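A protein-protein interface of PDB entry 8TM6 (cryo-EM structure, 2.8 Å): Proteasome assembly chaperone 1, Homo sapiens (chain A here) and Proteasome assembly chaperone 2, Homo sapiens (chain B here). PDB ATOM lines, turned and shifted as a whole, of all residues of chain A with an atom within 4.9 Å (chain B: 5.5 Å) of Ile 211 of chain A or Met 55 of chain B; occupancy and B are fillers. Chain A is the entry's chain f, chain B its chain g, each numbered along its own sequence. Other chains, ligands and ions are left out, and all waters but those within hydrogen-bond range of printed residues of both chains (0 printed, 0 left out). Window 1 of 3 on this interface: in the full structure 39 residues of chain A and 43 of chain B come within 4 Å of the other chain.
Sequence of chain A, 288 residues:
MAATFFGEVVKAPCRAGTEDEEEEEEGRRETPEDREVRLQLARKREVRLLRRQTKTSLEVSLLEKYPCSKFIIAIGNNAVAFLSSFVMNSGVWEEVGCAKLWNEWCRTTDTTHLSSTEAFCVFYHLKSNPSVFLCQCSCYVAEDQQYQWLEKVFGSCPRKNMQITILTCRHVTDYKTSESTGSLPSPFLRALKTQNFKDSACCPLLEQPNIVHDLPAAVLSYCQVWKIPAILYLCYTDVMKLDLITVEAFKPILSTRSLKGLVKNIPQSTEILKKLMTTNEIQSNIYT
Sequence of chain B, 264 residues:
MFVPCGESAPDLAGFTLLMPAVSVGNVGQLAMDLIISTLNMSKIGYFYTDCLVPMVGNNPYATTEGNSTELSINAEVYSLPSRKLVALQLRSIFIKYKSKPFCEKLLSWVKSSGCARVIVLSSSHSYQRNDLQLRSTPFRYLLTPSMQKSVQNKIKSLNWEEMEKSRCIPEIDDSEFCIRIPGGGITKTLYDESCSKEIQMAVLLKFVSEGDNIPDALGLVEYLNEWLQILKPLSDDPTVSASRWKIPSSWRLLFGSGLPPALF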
ATOM      1  N   GLN A 208     -24.462  23.111   3.102  1.00  0.00           N
ATOM      2  CA  GLN A 208     -25.559  22.481   3.833  1.00  0.00           C
ATOM      3  C   GLN A 208     -26.426  21.594   2.950  1.00  0.00           C
ATOM      4  O   GLN A 208     -26.698  20.447   3.346  1.00  0.00           O
ATOM      5  CB  GLN A 208     -26.398  23.563   4.521  1.00  0.00           C
ATOM      6  CG  GLN A 208     -25.604  24.436   5.481  1.00  0.00           C
ATOM      7  CD  GLN A 208     -24.996  23.645   6.624  1.00  0.00           C
ATOM      8  OE1 GLN A 208     -23.807  23.771   6.916  1.00  0.00           O
ATOM      9  NE2 GLN A 208     -25.812  22.828   7.280  1.00  0.00           N
ATOM     10  N   PRO A 209     -26.891  22.032   1.775  1.00  0.00           N
ATOM     11  CA  PRO A 209     -27.771  21.163   0.977  1.00  0.00           C
ATOM     12  C   PRO A 209     -27.055  19.998   0.314  1.00  0.00           C
ATOM     13  O   PRO A 209     -27.730  19.081  -0.169  1.00  0.00           O
ATOM     14  CB  PRO A 209     -28.359  22.121  -0.065  1.00  0.00           C
ATOM     15  CG  PRO A 209     -27.344  23.193  -0.200  1.00  0.00           C
ATOM     16  CD  PRO A 209     -26.723  23.360   1.157  1.00  0.00           C
ATOM     17  N   ASN A 210     -25.725  19.998   0.272  1.00  0.00           N
ATOM     18  CA  ASN A 210     -25.002  18.939  -0.419  1.00  0.00           C
ATOM     19  C   ASN A 210     -24.951  17.673   0.430  1.00  0.00           C
ATOM     20  O   ASN A 210     -24.592  17.711   1.611  1.00  0.00           O
ATOM     21  CB  ASN A 210     -23.588  19.404  -0.759  1.00  0.00           C
ATOM     22  CG  ASN A 210     -23.536  20.210  -2.041  1.00  0.00           C
ATOM     23  OD1 ASN A 210     -23.875  19.713  -3.114  1.00  0.00           O
ATOM     24  ND2 ASN A 210     -23.117  21.464  -1.934  1.00  0.00           N
ATOM     25  N   ILE A 211     -25.301  16.545  -0.187  1.00  0.00           N
ATOM     26  CA  ILE A 211     -25.403  15.257   0.493  1.00  0.00           C
ATOM     27  C   ILE A 211     -24.470  14.269  -0.195  1.00  0.00           C
ATOM     28  O   ILE A 211     -24.204  14.381  -1.396  1.00  0.00           O
ATOM     29  CB  ILE A 211     -26.857  14.726   0.481  1.00  0.00           C
ATOM     30  CG1 ILE A 211     -27.800  15.567   1.360  1.00  0.00           C
ATOM     31  CG2 ILE A 211     -26.903  13.268   0.929  1.00  0.00           C
ATOM     32  CD1 ILE A 211     -27.167  16.275   2.544  1.00  0.00           C
ATOM     33  N   VAL A 212     -23.970  13.302   0.574  1.00  0.00           N
ATOM     34  CA  VAL A 212     -23.166  12.196   0.061  1.00  0.00           C
ATOM     35  C   VAL A 212     -23.911  10.903   0.360  1.00  0.00           C
ATOM     36  O   VAL A 212     -24.350  10.683   1.495  1.00  0.00           O
ATOM     37  CB  VAL A 212     -21.761  12.181   0.690  1.00  0.00           C
ATOM     38  CG1 VAL A 212     -20.878  11.158  -0.005  1.00  0.00           C
ATOM     39  CG2 VAL A 212     -21.135  13.565   0.623  1.00  0.00           C
ATOM     40  N   HIS A 213     -24.058  10.050  -0.653  1.00  0.00           N
ATOM     41  CA  HIS A 213     -24.953   8.896  -0.574  1.00  0.00           C
ATOM     42  C   HIS A 213     -24.307   7.649  -1.176  1.00  0.00           C
ATOM     43  O   HIS A 213     -24.929   6.905  -1.937  1.00  0.00           O
ATOM     44  CB  HIS A 213     -26.275   9.211  -1.272  1.00  0.00           C
ATOM     45  CG  HIS A 213     -26.167   9.280  -2.764  1.00  0.00           C
ATOM     46  ND1 HIS A 213     -26.085   8.156  -3.557  1.00  0.00           N
ATOM     47  CD2 HIS A 213     -26.123  10.338  -3.608  1.00  0.00           C
ATOM     48  CE1 HIS A 213     -25.998   8.518  -4.824  1.00  0.00           C
ATOM     49  NE2 HIS A 213     -26.019   9.837  -4.882  1.00  0.00           N
ATOM     50  N   ALA A 217     -20.222   7.746   2.421  1.00  0.00           N
ATOM     51  CA  ALA A 217     -21.277   8.138   3.346  1.00  0.00           C
ATOM     52  C   ALA A 217     -21.544   7.041   4.366  1.00  0.00           C
ATOM     53  O   ALA A 217     -21.733   7.322   5.554  1.00  0.00           O
ATOM     54  CB  ALA A 217     -22.552   8.475   2.577  1.00  0.00           C
ATOM     55  N   SER A 221     -20.980   7.629   8.311  1.00  0.00           N
ATOM     56  CA  SER A 221     -22.102   7.467   9.230  1.00  0.00           C
ATOM     57  C   SER A 221     -21.790   6.425  10.296  1.00  0.00           C
ATOM     58  O   SER A 221     -22.113   6.616  11.474  1.00  0.00           O
ATOM     59  CB  SER A 221     -23.360   7.081   8.455  1.00  0.00           C
ATOM     60  OG  SER A 221     -23.200   5.827   7.815  1.00  0.00           O
ATOM     61  N   VAL B  53     -30.858   3.686   3.521  1.00  0.00           N
ATOM     62  CA  VAL B  53     -29.604   3.798   2.780  1.00  0.00           C
ATOM     63  C   VAL B  53     -28.757   4.886   3.432  1.00  0.00           C
ATOM     64  O   VAL B  53     -29.302   5.892   3.908  1.00  0.00           O
ATOM     65  CB  VAL B  53     -29.846   4.088   1.289  1.00  0.00           C
ATOM     66  CG1 VAL B  53     -30.691   2.988   0.667  1.00  0.00           C
ATOM     67  CG2 VAL B  53     -30.512   5.439   1.095  1.00  0.00           C
ATOM     68  N   PRO B  54     -27.437   4.735   3.475  1.00  0.00           N
ATOM     69  CA  PRO B  54     -26.607   5.683   4.221  1.00  0.00           C
ATOM     70  C   PRO B  54     -26.455   7.020   3.515  1.00  0.00           C
ATOM     71  O   PRO B  54     -26.502   7.119   2.287  1.00  0.00           O
ATOM     72  CB  PRO B  54     -25.261   4.958   4.321  1.00  0.00           C
ATOM     73  CG  PRO B  54     -25.210   4.103   3.104  1.00  0.00           C
ATOM     74  CD  PRO B  54     -26.628   3.728   2.766  1.00  0.00           C
ATOM     75  N   MET B  55     -26.269   8.059   4.325  1.00  0.00           N
ATOM     76  CA  MET B  55     -25.967   9.391   3.818  1.00  0.00           C
ATOM     77  C   MET B  55     -25.292  10.176   4.932  1.00  0.00           C
ATOM     78  O   MET B  55     -25.324   9.779   6.100  1.00  0.00           O
ATOM     79  CB  MET B  55     -27.223  10.119   3.333  1.00  0.00           C
ATOM     80  CG  MET B  55     -28.270  10.355   4.409  1.00  0.00           C
ATOM     81  SD  MET B  55     -29.132  11.917   4.160  1.00  0.00           S
ATOM     82  CE  MET B  55     -28.135  13.021   5.159  1.00  0.00           C
ATOM     83  N   VAL B  56     -24.682  11.301   4.556  1.00  0.00           N
ATOM     84  CA  VAL B  56     -24.020  12.177   5.512  1.00  0.00           C
ATOM     85  C   VAL B  56     -24.045  13.605   4.988  1.00  0.00           C
ATOM     86  O   VAL B  56     -24.223  13.855   3.795  1.00  0.00           O
ATOM     87  CB  VAL B  56     -22.566  11.742   5.797  1.00  0.00           C
ATOM     88  CG1 VAL B  56     -22.549  10.512   6.690  1.00  0.00           C
ATOM     89  CG2 VAL B  56     -21.819  11.486   4.497  1.00  0.00           C
ATOM     90  N   GLY B  57     -23.860  14.542   5.905  1.00  0.00           N
ATOM     91  CA  GLY B  57     -23.843  15.950   5.566  1.00  0.00           C
ATOM     92  C   GLY B  57     -24.025  16.796   6.802  1.00  0.00           C
ATOM     93  O   GLY B  57     -24.369  16.308   7.879  1.00  0.00           O
ATOM     94  N   SER B  72     -24.570  15.092  10.318  1.00  0.00           N
ATOM     95  CA  SER B  72     -25.805  14.342  10.489  1.00  0.00           C
ATOM     96  C   SER B  72     -25.778  13.089   9.623  1.00  0.00           C
ATOM     97  O   SER B  72     -24.994  12.977   8.677  1.00  0.00           O
ATOM     98  CB  SER B  72     -27.022  15.201  10.128  1.00  0.00           C
ATOM     99  OG  SER B  72     -28.229  14.510  10.395  1.00  0.00           O
ATOM    100  N   ILE B  73     -26.651  12.141   9.962  1.00  0.00           N
ATOM    101  CA  ILE B  73     -26.711  10.862   9.263  1.00  0.00           C
ATOM    102  C   ILE B  73     -28.108  10.648   8.696  1.00  0.00           C
ATOM    103  O   ILE B  73     -28.983  11.513   8.817  1.00  0.00           O
ATOM    104  CB  ILE B  73     -26.305   9.701  10.190  1.00  0.00           C
ATOM    105  CG1 ILE B  73     -27.246   9.603  11.392  1.00  0.00           C
ATOM    106  CG2 ILE B  73     -24.871   9.880  10.662  1.00  0.00           C
ATOM    107  CD1 ILE B  73     -27.388   8.200  11.926  1.00  0.00           C
ATOM    108  N   ASN B  74     -28.323   9.488   8.071  1.00  0.00           N
ATOM    109  CA  ASN B  74     -29.592   9.226   7.399  1.00  0.00           C
ATOM    110  C   ASN B  74     -30.758   9.218   8.380  1.00  0.00           C
ATOM    111  O   ASN B  74     -31.843   9.721   8.067  1.00  0.00           O
ATOM    112  CB  ASN B  74     -29.513   7.898   6.646  1.00  0.00           C
ATOM    113  CG  ASN B  74     -29.318   6.711   7.571  1.00  0.00           C
ATOM    114  OD1 ASN B  74     -29.195   6.868   8.785  1.00  0.00           O
ATOM    115  ND2 ASN B  74     -29.282   5.516   6.997  1.00  0.00           N
ATOM    116  N   ARG B  91     -33.766  10.572   6.647  1.00  0.00           N
ATOM    117  CA  ARG B  91     -33.255  11.490   5.636  1.00  0.00           C
ATOM    118  C   ARG B  91     -32.843  10.769   4.357  1.00  0.00           C
ATOM    119  O   ARG B  91     -32.069  11.314   3.566  1.00  0.00           O
ATOM    120  CB  ARG B  91     -32.072  12.281   6.199  1.00  0.00           C
ATOM    121  CG  ARG B  91     -32.432  13.644   6.751  1.00  0.00           C
ATOM    122  CD  ARG B  91     -31.184  14.425   7.121  1.00  0.00           C
ATOM    123  NE  ARG B  91     -31.412  15.324   8.245  1.00  0.00           N
ATOM    124  CZ  ARG B  91     -31.395  14.953   9.518  1.00  0.00           C
ATOM    125  NH1 ARG B  91     -31.166  13.698   9.871  1.00  0.00           N
ATOM    126  NH2 ARG B  91     -31.615  15.863  10.463  1.00  0.00           N
ATOM    127  N   SER B  92     -33.345   9.559   4.130  1.00  0.00           N
ATOM    128  CA  SER B  92     -32.919   8.764   2.986  1.00  0.00           C
ATOM    129  C   SER B  92     -34.067   7.860   2.551  1.00  0.00           C
ATOM    130  O   SER B  92     -35.196   7.979   3.036  1.00  0.00           O
ATOM    131  CB  SER B  92     -31.652   7.971   3.333  1.00  0.00           C
ATOM    132  OG  SER B  92     -30.492   8.724   3.044  1.00  0.00           O
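The backbone carbonyl oxygen of Val 212 of chain A sits at hydrogen-bond distance from the backbone NH of Val 56 of chain B (3.1 Å).
The backbone carbonyl oxygen of Ala 217 of chain A sits at hydrogen-bond distance from the side-chain hydroxyl of Ser 221 of chain A, 3.1 Å away.
SD of Met 55 of chain B sits close to OG of Ser 92 of chain B, 3.6 Å away.
The backbone carbonyl oxygen (O) of Ile 73 of chain B lies within hydrogen-bond range of the guanidinium group (NH1) of Arg 91 of chain B, at 3.3 Å.
Among the printed residues, pairs that only touch across the chains: Val 212 of chain A with Met 55 of chain B, Ala 217 of chain A with Val 56 of chain B, Ser 221 of chain A with Val 56 of chain B, His 213 of chain A with Pro 54 of chain B, Ala 217 of chain A with Met 55 of chain B, Ile 211 of chain A with Val 56 of chain B, Ser 221 of chain A with Ile 73 of chain B and Ile 211 of chain A with Met 55 of chain B.
Ile 211 of chain A touches just these residues of chain B: Met 55 and Val 56.
Met 55 of chain B touches just these residues of chain A: Ile 211, Val 212 and Ala 217.
Printed residues of chain B within 4 Å of His 213 of chain A: Pro 54 (3.7 Å).
Printed residues of chain A within 4 Å of Pro 54 of chain B: His 213.
Printed residues of chain A within 4 Å of Ile 73 of chain B: Ser 221.
Ser 92 of chain B touches none of the printed residues of chain A.
Gly 57 of chain B touches none of the printed residues of chain A.
The nearest residue of chain A that does not touch Met 55 of chain B is Ser 221 of chain A (4.1 Å).
Of the 8 printed residues of chain A, 5 touch a printed residue of chain B.
Hydrophobic or aromatic side chains of chain B within 4 Å of the printed part of chain A: Met 55, Val 56 and Ile 73.
Among the printed residues, no Asp or Glu carboxylate lies within 4 Å of a Lys or Arg side-chain nitrogen of the other chain.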
